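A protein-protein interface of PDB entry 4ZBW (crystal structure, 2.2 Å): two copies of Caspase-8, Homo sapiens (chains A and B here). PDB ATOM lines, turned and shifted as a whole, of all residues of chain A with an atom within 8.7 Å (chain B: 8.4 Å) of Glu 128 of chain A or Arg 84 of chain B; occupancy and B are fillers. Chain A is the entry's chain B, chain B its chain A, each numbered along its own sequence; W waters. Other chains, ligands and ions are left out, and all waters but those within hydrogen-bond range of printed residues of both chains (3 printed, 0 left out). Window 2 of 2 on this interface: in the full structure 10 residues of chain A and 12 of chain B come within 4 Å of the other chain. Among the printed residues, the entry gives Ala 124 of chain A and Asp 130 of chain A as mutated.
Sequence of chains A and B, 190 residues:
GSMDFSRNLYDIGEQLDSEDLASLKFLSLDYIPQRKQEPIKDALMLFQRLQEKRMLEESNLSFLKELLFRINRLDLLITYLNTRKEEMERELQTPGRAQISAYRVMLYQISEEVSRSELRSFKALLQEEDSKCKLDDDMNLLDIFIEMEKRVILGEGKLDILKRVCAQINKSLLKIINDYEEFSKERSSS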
ATOM      1  N   SER A 121     -31.938  14.423  -3.245  1.00  0.00           N
ATOM      2  CA  SER A 121     -30.528  14.596  -3.583  1.00  0.00           C
ATOM      3  C   SER A 121     -29.638  13.779  -2.647  1.00  0.00           C
ATOM      4  O   SER A 121     -28.659  13.176  -3.083  1.00  0.00           O
ATOM      5  CB  SER A 121     -30.134  16.072  -3.533  1.00  0.00           C
ATOM      6  OG  SER A 121     -30.869  16.826  -4.482  1.00  0.00           O
ATOM      7  N   PHE A 122     -29.989  13.755  -1.363  1.00  0.00           N
ATOM      8  CA  PHE A 122     -29.245  12.965  -0.390  1.00  0.00           C
ATOM      9  C   PHE A 122     -29.243  11.501  -0.808  1.00  0.00           C
ATOM     10  O   PHE A 122     -28.198  10.851  -0.808  1.00  0.00           O
ATOM     11  CB  PHE A 122     -29.839  13.106   1.017  1.00  0.00           C
ATOM     12  CG  PHE A 122     -28.899  12.689   2.116  1.00  0.00           C
ATOM     13  CD1 PHE A 122     -28.691  11.345   2.402  1.00  0.00           C
ATOM     14  CD2 PHE A 122     -28.231  13.641   2.872  1.00  0.00           C
ATOM     15  CE1 PHE A 122     -27.824  10.958   3.417  1.00  0.00           C
ATOM     16  CE2 PHE A 122     -27.363  13.262   3.885  1.00  0.00           C
ATOM     17  CZ  PHE A 122     -27.160  11.916   4.156  1.00  0.00           C
ATOM     18  N   LYS A 123     -30.413  10.992  -1.182  1.00  0.00           N
ATOM     19  CA  LYS A 123     -30.507   9.603  -1.617  1.00  0.00           C
ATOM     20  C   LYS A 123     -29.652   9.334  -2.856  1.00  0.00           C
ATOM     21  O   LYS A 123     -28.898   8.358  -2.887  1.00  0.00           O
ATOM     22  CB  LYS A 123     -31.967   9.222  -1.878  1.00  0.00           C
ATOM     23  CG  LYS A 123     -32.814   9.274  -0.615  1.00  0.00           C
ATOM     24  CD  LYS A 123     -34.227   8.752  -0.817  1.00  0.00           C
ATOM     25  CE  LYS A 123     -35.003   8.831   0.495  1.00  0.00           C
ATOM     26  NZ  LYS A 123     -36.365   8.243   0.415  1.00  0.00           N
ATOM     27  N   ALA A 124     -29.735  10.210  -3.858  1.00  0.00           N
ATOM     28  CA  ALA A 124     -28.950  10.018  -5.083  1.00  0.00           C
ATOM     29  C   ALA A 124     -27.440  10.033  -4.810  1.00  0.00           C
ATOM     30  O   ALA A 124     -26.695   9.158  -5.274  1.00  0.00           O
ATOM     31  CB  ALA A 124     -29.309  11.081  -6.111  1.00  0.00           C
ATOM     32  N   LEU A 125     -26.999  11.021  -4.040  1.00  0.00           N
ATOM     33  CA  LEU A 125     -25.582  11.191  -3.739  1.00  0.00           C
ATOM     34  C   LEU A 125     -25.047  10.047  -2.885  1.00  0.00           C
ATOM     35  O   LEU A 125     -23.911   9.604  -3.071  1.00  0.00           O
ATOM     36  CB  LEU A 125     -25.345  12.531  -3.035  1.00  0.00           C
ATOM     37  CG  LEU A 125     -25.592  13.778  -3.888  1.00  0.00           C
ATOM     38  CD1 LEU A 125     -25.582  15.029  -3.026  1.00  0.00           C
ATOM     39  CD2 LEU A 125     -24.560  13.880  -4.999  1.00  0.00           C
ATOM     40  N   LEU A 126     -25.861   9.568  -1.949  1.00  0.00           N
ATOM     41  CA  LEU A 126     -25.464   8.428  -1.134  1.00  0.00           C
ATOM     42  C   LEU A 126     -25.359   7.178  -2.001  1.00  0.00           C
ATOM     43  O   LEU A 126     -24.436   6.379  -1.837  1.00  0.00           O
ATOM     44  CB  LEU A 126     -26.442   8.201   0.019  1.00  0.00           C
ATOM     45  CG  LEU A 126     -26.148   6.980   0.899  1.00  0.00           C
ATOM     46  CD1 LEU A 126     -24.768   7.084   1.532  1.00  0.00           C
ATOM     47  CD2 LEU A 126     -27.217   6.816   1.973  1.00  0.00           C
ATOM     48  N   GLN A 127     -26.294   7.015  -2.937  1.00  0.00           N
ATOM     49  CA  GLN A 127     -26.232   5.874  -3.846  1.00  0.00           C
ATOM     50  C   GLN A 127     -24.982   5.954  -4.713  1.00  0.00           C
ATOM     51  O   GLN A 127     -24.445   4.929  -5.132  1.00  0.00           O
ATOM     52  CB  GLN A 127     -27.477   5.802  -4.735  1.00  0.00           C
ATOM     53  CG  GLN A 127     -28.768   5.470  -4.001  1.00  0.00           C
ATOM     54  CD  GLN A 127     -29.966   5.412  -4.934  1.00  0.00           C
ATOM     55  OE1 GLN A 127     -30.102   4.483  -5.732  1.00  0.00           O
ATOM     56  NE2 GLN A 127     -30.843   6.406  -4.836  1.00  0.00           N
ATOM     57  N   GLU A 128     -24.512   7.173  -4.969  1.00  0.00           N
ATOM     58  CA  GLU A 128     -23.214   7.348  -5.617  1.00  0.00           C
ATOM     59  C   GLU A 128     -22.060   6.930  -4.709  1.00  0.00           C
ATOM     60  O   GLU A 128     -21.118   6.271  -5.152  1.00  0.00           O
ATOM     61  CB  GLU A 128     -23.016   8.801  -6.049  1.00  0.00           C
ATOM     62  CG  GLU A 128     -23.878   9.239  -7.213  1.00  0.00           C
ATOM     63  CD  GLU A 128     -23.558  10.650  -7.652  1.00  0.00           C
ATOM     64  OE1 GLU A 128     -22.579  11.220  -7.129  1.00  0.00           O
ATOM     65  OE2 GLU A 128     -24.283  11.186  -8.514  1.00  0.00           O
ATOM     66  N   GLU A 129     -22.139   7.317  -3.438  1.00  0.00           N
ATOM     67  CA  GLU A 129     -21.041   7.101  -2.497  1.00  0.00           C
ATOM     68  C   GLU A 129     -20.943   5.667  -1.988  1.00  0.00           C
ATOM     69  O   GLU A 129     -19.859   5.203  -1.631  1.00  0.00           O
ATOM     70  CB  GLU A 129     -21.180   8.046  -1.299  1.00  0.00           C
ATOM     71  CG  GLU A 129     -20.987   9.518  -1.630  1.00  0.00           C
ATOM     72  CD  GLU A 129     -19.537   9.879  -1.878  1.00  0.00           C
ATOM     73  OE1 GLU A 129     -18.650   9.116  -1.442  1.00  0.00           O
ATOM     74  OE2 GLU A 129     -19.284  10.926  -2.511  1.00  0.00           O
ATOM     75  N   ASP A 130     -22.071   4.967  -1.949  1.00  0.00           N
ATOM     76  CA  ASP A 130     -22.092   3.623  -1.385  1.00  0.00           C
ATOM     77  C   ASP A 130     -23.211   2.783  -1.999  1.00  0.00           C
ATOM     78  O   ASP A 130     -24.240   3.316  -2.413  1.00  0.00           O
ATOM     79  CB  ASP A 130     -22.245   3.709   0.137  1.00  0.00           C
ATOM     80  CG  ASP A 130     -22.503   2.367   0.777  1.00  0.00           C
ATOM     81  OD1 ASP A 130     -21.521   1.659   1.085  1.00  0.00           O
ATOM     82  OD2 ASP A 130     -23.688   2.024   0.973  1.00  0.00           O
ATOM     83  N   SER A 131     -23.008   1.469  -2.059  1.00  0.00           N
ATOM     84  CA  SER A 131     -24.003   0.574  -2.642  1.00  0.00           C
ATOM     85  C   SER A 131     -24.543  -0.460  -1.656  1.00  0.00           C
ATOM     86  O   SER A 131     -25.436  -1.238  -1.997  1.00  0.00           O
ATOM     87  CB  SER A 131     -23.417  -0.146  -3.859  1.00  0.00           C
ATOM     88  OG  SER A 131     -23.221   0.751  -4.937  1.00  0.00           O
ATOM     89  N   LEU A 135     -31.936   1.486  -0.041  1.00  0.00           N
ATOM     90  CA  LEU A 135     -32.717   2.712   0.014  1.00  0.00           C
ATOM     91  C   LEU A 135     -33.988   2.623  -0.819  1.00  0.00           C
ATOM     92  O   LEU A 135     -33.973   2.123  -1.944  1.00  0.00           O
ATOM     93  CB  LEU A 135     -31.875   3.898  -0.464  1.00  0.00           C
ATOM     94  CG  LEU A 135     -30.564   4.140   0.285  1.00  0.00           C
ATOM     95  CD1 LEU A 135     -29.798   5.301  -0.330  1.00  0.00           C
ATOM     96  CD2 LEU A 135     -30.828   4.383   1.763  1.00  0.00           C
ATOM     97  N   ILE A 161     -18.489  10.005   4.775  1.00  0.00           N
ATOM     98  CA  ILE A 161     -19.523   9.869   3.760  1.00  0.00           C
ATOM     99  C   ILE A 161     -20.635  10.884   4.003  1.00  0.00           C
ATOM    100  O   ILE A 161     -21.134  11.506   3.059  1.00  0.00           O
ATOM    101  CB  ILE A 161     -20.092   8.439   3.734  1.00  0.00           C
ATOM    102  CG1 ILE A 161     -18.992   7.457   3.327  1.00  0.00           C
ATOM    103  CG2 ILE A 161     -21.267   8.343   2.772  1.00  0.00           C
ATOM    104  CD1 ILE A 161     -19.445   6.019   3.238  1.00  0.00           C
ATOM    105  N   ARG A 164     -19.255  14.186   2.751  1.00  0.00           N
ATOM    106  CA  ARG A 164     -19.116  14.220   1.300  1.00  0.00           C
ATOM    107  C   ARG A 164     -20.474  14.376   0.629  1.00  0.00           C
ATOM    108  O   ARG A 164     -20.597  15.062  -0.383  1.00  0.00           O
ATOM    109  CB  ARG A 164     -18.408  12.967   0.784  1.00  0.00           C
ATOM    110  CG  ARG A 164     -16.914  12.963   1.050  1.00  0.00           C
ATOM    111  CD  ARG A 164     -16.177  12.042   0.090  1.00  0.00           C
ATOM    112  NE  ARG A 164     -16.532  10.638   0.274  1.00  0.00           N
ATOM    113  CZ  ARG A 164     -15.909   9.817   1.115  1.00  0.00           C
ATOM    114  NH1 ARG A 164     -14.902  10.262   1.855  1.00  0.00           N
ATOM    115  NH2 ARG A 164     -16.294   8.551   1.216  1.00  0.00           N
ATOM    116  N   VAL A 165     -21.496  13.747   1.201  1.00  0.00           N
ATOM    117  CA  VAL A 165     -22.850  13.923   0.694  1.00  0.00           C
ATOM    118  C   VAL A 165     -23.361  15.339   0.980  1.00  0.00           C
ATOM    119  O   VAL A 165     -23.777  16.053   0.063  1.00  0.00           O
ATOM    120  CB  VAL A 165     -23.822  12.890   1.308  1.00  0.00           C
ATOM    121  CG1 VAL A 165     -25.262  13.222   0.940  1.00  0.00           C
ATOM    122  CG2 VAL A 165     -23.458  11.483   0.852  1.00  0.00           C
ATOM    123  N   GLN A 168     -22.349  18.553  -0.957  1.00  0.00           N
ATOM    124  CA  GLN A 168     -22.867  18.710  -2.308  1.00  0.00           C
ATOM    125  C   GLN A 168     -24.330  19.140  -2.303  1.00  0.00           C
ATOM    126  O   GLN A 168     -24.925  19.356  -3.358  1.00  0.00           O
ATOM    127  CB  GLN A 168     -22.710  17.407  -3.093  1.00  0.00           C
ATOM    128  CG  GLN A 168     -21.297  16.855  -3.104  1.00  0.00           C
ATOM    129  CD  GLN A 168     -21.186  15.557  -3.884  1.00  0.00           C
ATOM    130  OE1 GLN A 168     -21.247  15.551  -5.115  1.00  0.00           O
ATOM    131  NE2 GLN A 168     -21.038  14.446  -3.169  1.00  0.00           N
ATOM    132  N   LYS B  65     -15.431  28.344 -11.582  1.00  0.00           N
ATOM    133  CA  LYS B  65     -15.559  26.948 -11.183  1.00  0.00           C
ATOM    134  C   LYS B  65     -14.421  26.533 -10.252  1.00  0.00           C
ATOM    135  O   LYS B  65     -14.653  25.879  -9.236  1.00  0.00           O
ATOM    136  CB  LYS B  65     -15.591  26.038 -12.414  1.00  0.00           C
ATOM    137  CG  LYS B  65     -16.870  26.133 -13.239  1.00  0.00           C
ATOM    138  CD  LYS B  65     -16.770  25.274 -14.488  1.00  0.00           C
ATOM    139  CE  LYS B  65     -18.063  25.287 -15.285  1.00  0.00           C
ATOM    140  NZ  LYS B  65     -17.946  24.479 -16.541  1.00  0.00           N
ATOM    141  N   PHE B  69     -14.873  25.421  -6.379  1.00  0.00           N
ATOM    142  CA  PHE B  69     -14.371  24.102  -6.007  1.00  0.00           C
ATOM    143  C   PHE B  69     -13.384  24.196  -4.848  1.00  0.00           C
ATOM    144  O   PHE B  69     -13.466  23.425  -3.895  1.00  0.00           O
ATOM    145  CB  PHE B  69     -13.708  23.419  -7.207  1.00  0.00           C
ATOM    146  CG  PHE B  69     -13.129  22.063  -6.897  1.00  0.00           C
ATOM    147  CD1 PHE B  69     -13.956  20.965  -6.713  1.00  0.00           C
ATOM    148  CD2 PHE B  69     -11.759  21.883  -6.806  1.00  0.00           C
ATOM    149  CE1 PHE B  69     -13.427  19.713  -6.436  1.00  0.00           C
ATOM    150  CE2 PHE B  69     -11.222  20.635  -6.532  1.00  0.00           C
ATOM    151  CZ  PHE B  69     -12.058  19.548  -6.346  1.00  0.00           C
ATOM    152  N   LEU B  74     -19.379  22.730  -3.335  1.00  0.00           N
ATOM    153  CA  LEU B  74     -19.791  21.739  -4.329  1.00  0.00           C
ATOM    154  C   LEU B  74     -21.290  21.819  -4.606  1.00  0.00           C
ATOM    155  O   LEU B  74     -21.753  21.528  -5.721  1.00  0.00           O
ATOM    156  CB  LEU B  74     -19.415  20.329  -3.860  1.00  0.00           C
ATOM    157  CG  LEU B  74     -17.951  20.113  -3.465  1.00  0.00           C
ATOM    158  CD1 LEU B  74     -17.716  18.687  -2.970  1.00  0.00           C
ATOM    159  CD2 LEU B  74     -17.023  20.446  -4.631  1.00  0.00           C
ATOM    160  N   LEU B  77     -21.745  24.492  -7.210  1.00  0.00           N
ATOM    161  CA  LEU B  77     -21.260  23.987  -8.487  1.00  0.00           C
ATOM    162  C   LEU B  77     -22.336  23.136  -9.142  1.00  0.00           C
ATOM    163  O   LEU B  77     -22.655  23.324 -10.323  1.00  0.00           O
ATOM    164  CB  LEU B  77     -19.976  23.177  -8.300  1.00  0.00           C
ATOM    165  CG  LEU B  77     -18.698  24.002  -8.139  1.00  0.00           C
ATOM    166  CD1 LEU B  77     -17.549  23.132  -7.658  1.00  0.00           C
ATOM    167  CD2 LEU B  77     -18.343  24.694  -9.453  1.00  0.00           C
ATOM    168  N   ILE B  78     -22.920  22.228  -8.360  1.00  0.00           N
ATOM    169  CA  ILE B  78     -23.997  21.384  -8.869  1.00  0.00           C
ATOM    170  C   ILE B  78     -25.231  22.202  -9.244  1.00  0.00           C
ATOM    171  O   ILE B  78     -25.713  22.125 -10.373  1.00  0.00           O
ATOM    172  CB  ILE B  78     -24.420  20.311  -7.844  1.00  0.00           C
ATOM    173  CG1 ILE B  78     -23.296  19.299  -7.633  1.00  0.00           C
ATOM    174  CG2 ILE B  78     -25.688  19.604  -8.310  1.00  0.00           C
ATOM    175  CD1 ILE B  78     -23.583  18.287  -6.547  1.00  0.00           C
ATOM    176  N   THR B  79     -25.730  22.991  -8.296  1.00  0.00           N
ATOM    177  CA  THR B  79     -26.984  23.717  -8.484  1.00  0.00           C
ATOM    178  C   THR B  79     -26.949  24.714  -9.644  1.00  0.00           C
ATOM    179  O   THR B  79     -27.837  24.716 -10.499  1.00  0.00           O
ATOM    180  CB  THR B  79     -27.379  24.481  -7.206  1.00  0.00           C
ATOM    181  OG1 THR B  79     -27.544  23.557  -6.124  1.00  0.00           O
ATOM    182  CG2 THR B  79     -28.682  25.245  -7.417  1.00  0.00           C
ATOM    183  N   LEU B  81     -23.995  25.594 -11.669  1.00  0.00           N
ATOM    184  CA  LEU B  81     -23.030  25.424 -12.751  1.00  0.00           C
ATOM    185  C   LEU B  81     -23.025  24.007 -13.320  1.00  0.00           C
ATOM    186  O   LEU B  81     -22.240  23.701 -14.220  1.00  0.00           O
ATOM    187  CB  LEU B  81     -21.629  25.810 -12.275  1.00  0.00           C
ATOM    188  CG  LEU B  81     -21.454  27.303 -11.988  1.00  0.00           C
ATOM    189  CD1 LEU B  81     -20.059  27.596 -11.470  1.00  0.00           C
ATOM    190  CD2 LEU B  81     -21.748  28.125 -13.239  1.00  0.00           C
ATOM    191  N   ASN B  82     -23.911  23.162 -12.799  1.00  0.00           N
ATOM    192  CA  ASN B  82     -24.045  21.780 -13.254  1.00  0.00           C
ATOM    193  C   ASN B  82     -22.693  21.090 -13.381  1.00  0.00           C
ATOM    194  O   ASN B  82     -22.401  20.446 -14.387  1.00  0.00           O
ATOM    195  CB  ASN B  82     -24.780  21.735 -14.598  1.00  0.00           C
ATOM    196  CG  ASN B  82     -25.318  20.354 -14.923  1.00  0.00           C
ATOM    197  OD1 ASN B  82     -25.657  19.581 -14.028  1.00  0.00           O
ATOM    198  ND2 ASN B  82     -25.389  20.036 -16.212  1.00  0.00           N
ATOM    199  N   THR B  83     -21.870  21.232 -12.350  1.00  0.00           N
ATOM    200  CA  THR B  83     -20.511  20.714 -12.391  1.00  0.00           C
ATOM    201  C   THR B  83     -20.225  19.851 -11.168  1.00  0.00           C
ATOM    202  O   THR B  83     -20.422  20.283 -10.032  1.00  0.00           O
ATOM    203  CB  THR B  83     -19.478  21.856 -12.465  1.00  0.00           C
ATOM    204  OG1 THR B  83     -19.725  22.657 -13.627  1.00  0.00           O
ATOM    205  CG2 THR B  83     -18.067  21.294 -12.529  1.00  0.00           C
ATOM    206  N   ARG B  84     -19.760  18.630 -11.418  1.00  0.00           N
ATOM    207  CA  ARG B  84     -19.467  17.675 -10.359  1.00  0.00           C
ATOM    208  C   ARG B  84     -18.022  17.787  -9.887  1.00  0.00           C
ATOM    209  O   ARG B  84     -17.156  18.291 -10.607  1.00  0.00           O
ATOM    210  CB  ARG B  84     -19.745  16.241 -10.830  1.00  0.00           C
ATOM    211  CG  ARG B  84     -21.176  15.984 -11.297  1.00  0.00           C
ATOM    212  CD  ARG B  84     -22.198  16.324 -10.218  1.00  0.00           C
ATOM    213  NE  ARG B  84     -21.924  15.652  -8.946  1.00  0.00           N
ATOM    214  CZ  ARG B  84     -22.336  14.426  -8.633  1.00  0.00           C
ATOM    215  NH1 ARG B  84     -23.044  13.714  -9.500  1.00  0.00           N
ATOM    216  NH2 ARG B  84     -22.037  13.910  -7.448  1.00  0.00           N
ATOM    217  N   LYS B  85     -17.780  17.305  -8.672  1.00  0.00           N
ATOM    218  CA  LYS B  85     -16.458  17.293  -8.050  1.00  0.00           C
ATOM    219  C   LYS B  85     -15.433  16.497  -8.861  1.00  0.00           C
ATOM    220  O   LYS B  85     -14.270  16.898  -8.989  1.00  0.00           O
ATOM    221  CB  LYS B  85     -16.585  16.693  -6.644  1.00  0.00           C
ATOM    222  CG  LYS B  85     -15.389  15.875  -6.179  1.00  0.00           C
ATOM    223  CD  LYS B  85     -15.543  15.439  -4.728  1.00  0.00           C
ATOM    224  CE  LYS B  85     -14.431  14.483  -4.319  1.00  0.00           C
ATOM    225  NZ  LYS B  85     -14.645  13.897  -2.966  1.00  0.00           N
ATOM    226  N   GLU B  86     -15.888  15.382  -9.424  1.00  0.00           N
ATOM    227  CA  GLU B  86     -15.055  14.503 -10.237  1.00  0.00           C
ATOM    228  C   GLU B  86     -14.457  15.233 -11.441  1.00  0.00           C
ATOM    229  O   GLU B  86     -13.263  15.095 -11.744  1.00  0.00           O
ATOM    230  CB  GLU B  86     -15.883  13.299 -10.695  1.00  0.00           C
ATOM    231  CG  GLU B  86     -15.230  12.418 -11.745  1.00  0.00           C
ATOM    232  CD  GLU B  86     -16.097  11.223 -12.107  1.00  0.00           C
ATOM    233  OE1 GLU B  86     -17.265  11.180 -11.665  1.00  0.00           O
ATOM    234  OE2 GLU B  86     -15.616  10.330 -12.837  1.00  0.00           O
ATOM    235  N   GLU B  87     -15.292  16.030 -12.104  1.00  0.00           N
ATOM    236  CA  GLU B  87     -14.859  16.787 -13.267  1.00  0.00           C
ATOM    237  C   GLU B  87     -13.817  17.825 -12.874  1.00  0.00           C
ATOM    238  O   GLU B  87     -12.795  17.963 -13.540  1.00  0.00           O
ATOM    239  CB  GLU B  87     -16.046  17.473 -13.943  1.00  0.00           C
ATOM    240  CG  GLU B  87     -15.656  18.354 -15.125  1.00  0.00           C
ATOM    241  CD  GLU B  87     -16.806  19.202 -15.627  1.00  0.00           C
ATOM    242  OE1 GLU B  87     -17.916  19.096 -15.067  1.00  0.00           O
ATOM    243  OE2 GLU B  87     -16.600  19.983 -16.579  1.00  0.00           O
ATOM    244  N   MET B  88     -14.078  18.550 -11.791  1.00  0.00           N
ATOM    245  CA  MET B  88     -13.155  19.580 -11.331  1.00  0.00           C
ATOM    246  C   MET B  88     -11.809  18.984 -10.934  1.00  0.00           C
ATOM    247  O   MET B  88     -10.763  19.568 -11.201  1.00  0.00           O
ATOM    248  CB  MET B  88     -13.750  20.356 -10.154  1.00  0.00           C
ATOM    249  CG  MET B  88     -14.975  21.177 -10.520  1.00  0.00           C
ATOM    250  SD  MET B  88     -14.647  22.333 -11.869  1.00  0.00           S
ATOM    251  CE  MET B  88     -13.275  23.276 -11.203  1.00  0.00           C
ATOM    252  N   GLU B  89     -11.839  17.813 -10.306  1.00  0.00           N
ATOM    253  CA  GLU B  89     -10.609  17.122  -9.938  1.00  0.00           C
ATOM    254  C   GLU B  89      -9.822  16.719 -11.181  1.00  0.00           C
ATOM    255  O   GLU B  89      -8.615  16.984 -11.281  1.00  0.00           O
ATOM    256  CB  GLU B  89     -10.925  15.905  -9.074  1.00  0.00           C
ATOM    257  CG  GLU B  89     -10.909  16.215  -7.591  1.00  0.00           C
ATOM    258  CD  GLU B  89     -11.643  15.178  -6.773  1.00  0.00           C
ATOM    259  OE1 GLU B  89     -12.244  14.261  -7.372  1.00  0.00           O
ATOM    260  OE2 GLU B  89     -11.621  15.286  -5.529  1.00  0.00           O
ATOM    261  N   ARG B  90     -10.513  16.098 -12.135  1.00  0.00           N
ATOM    262  CA  ARG B  90      -9.877  15.684 -13.384  1.00  0.00           C
ATOM    263  C   ARG B  90      -9.262  16.876 -14.118  1.00  0.00           C
ATOM    264  O   ARG B  90      -8.150  16.793 -14.636  1.00  0.00           O
ATOM    265  CB  ARG B  90     -10.892  14.964 -14.279  1.00  0.00           C
ATOM    266  CG  ARG B  90     -10.365  14.561 -15.648  1.00  0.00           C
ATOM    267  CD  ARG B  90     -11.479  13.955 -16.497  1.00  0.00           C
ATOM    268  NE  ARG B  90     -12.620  14.858 -16.636  1.00  0.00           N
ATOM    269  CZ  ARG B  90     -12.814  15.682 -17.660  1.00  0.00           C
ATOM    270  NH1 ARG B  90     -11.933  15.735 -18.651  1.00  0.00           N
ATOM    271  NH2 ARG B  90     -13.887  16.461 -17.688  1.00  0.00           N
ATOM    272  N   GLU B  91      -9.979  17.994 -14.135  1.00  0.00           N
ATOM    273  CA  GLU B  91      -9.518  19.184 -14.834  1.00  0.00           C
ATOM    274  C   GLU B  91      -8.316  19.816 -14.144  1.00  0.00           C
ATOM    275  O   GLU B  91      -7.331  20.162 -14.792  1.00  0.00           O
ATOM    276  CB  GLU B  91     -10.648  20.208 -14.952  1.00  0.00           C
ATOM    277  CG  GLU B  91     -11.670  19.878 -16.019  1.00  0.00           C
ATOM    278  CD  GLU B  91     -11.220  20.334 -17.393  1.00  0.00           C
ATOM    279  OE1 GLU B  91     -11.434  21.517 -17.724  1.00  0.00           O
ATOM    280  OE2 GLU B  91     -10.643  19.514 -18.137  1.00  0.00           O
HETATM  281  O   HOH W   1     -26.625  21.074  -4.697  1.00  0.00           O
HETATM  282  O   HOH W   2     -20.146  17.114  -7.040  1.00  0.00           O
HETATM  283  O   HOH W   3     -17.809  13.157  -3.165  1.00  0.00           O
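OE1 of Glu 129 of chain A lies within salt-bridge range of NE of Arg 164 of chain A, at 3.1 Å.
NE2 of Gln 168 of chain A lies within hydrogen-bond range of O of Arg 164 of chain A (2.9 Å).
The guanidinium group of Arg 84 of chain B is in salt-bridge range of the side-chain carboxylate of Glu 128 of chain A, 2.8 Å away.
The guanidinium group (NH2) of Arg 84 of chain B is in hydrogen-bond range of the side-chain amide oxygen (OE1) of Gln 168 of chain A (3.0 Å).
Water W2 lies within hydrogen-bond range of OE1 of Gln 168 of chain A (2.7 Å), N of Lys 85 of chain B (2.9 Å) and NE of Arg 84 of chain B (3.0 Å).
Water W3 lies within hydrogen-bond range of OE2 of Glu 129 of chain A (2.8 Å), NZ of Lys 85 of chain B (3.3 Å) and NE2 of Gln 168 of chain A (3.5 Å).
Water W1 bridges O of Gln 168 of chain A (2.8 Å) and OG1 of Thr 79 of chain B (3.0 Å).
Of the 16 printed residues of chain A, 4 touch a printed residue of chain B.
Hydrophobic or aromatic side chains of chain A that line the printed part of chain B: Leu 125.
Of the 17 printed residues of chain B, 3 touch a printed residue of chain A.
Hydrophobic or aromatic side chains of chain B that line the printed part of chain A: Ile 78.
Among the printed residues, 5 pairs touch across the chains.
Among the printed residues, Asp or Glu carboxylates within 4 Å of a Lys or Arg side-chain nitrogen of the other chain: Glu 128 of chain A with Arg 84 of chain B.
Among the printed residues, pairs that only touch across the chains: Leu 125 of chain A with Arg 84 of chain B, Gln 168 of chain A with Ile 78 of chain B and Arg 164 of chain A with Lys 85 of chain B.
No position is printed for both chains.
Of the 5 pairs that touch across the chains among the printed residues, none has its exchanged pair printed and touching as well.
Leu 126 of chain A touches none of the printed residues of chain B.
Of the printed residues of chain A, Ile 78 of chain B touches Gln 168.
Arg 84 of chain B touches just these residues of chain A: Leu 125, Glu 128 and Gln 168.
Of the printed residues of chain A, Lys 85 of chain B touches Arg 164.
Met 88 of chain B touches none of the printed residues of chain A.
The nearest residue of chain B that does not touch Glu 128 of chain A is Glu 86 of chain B (7.0 Å).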
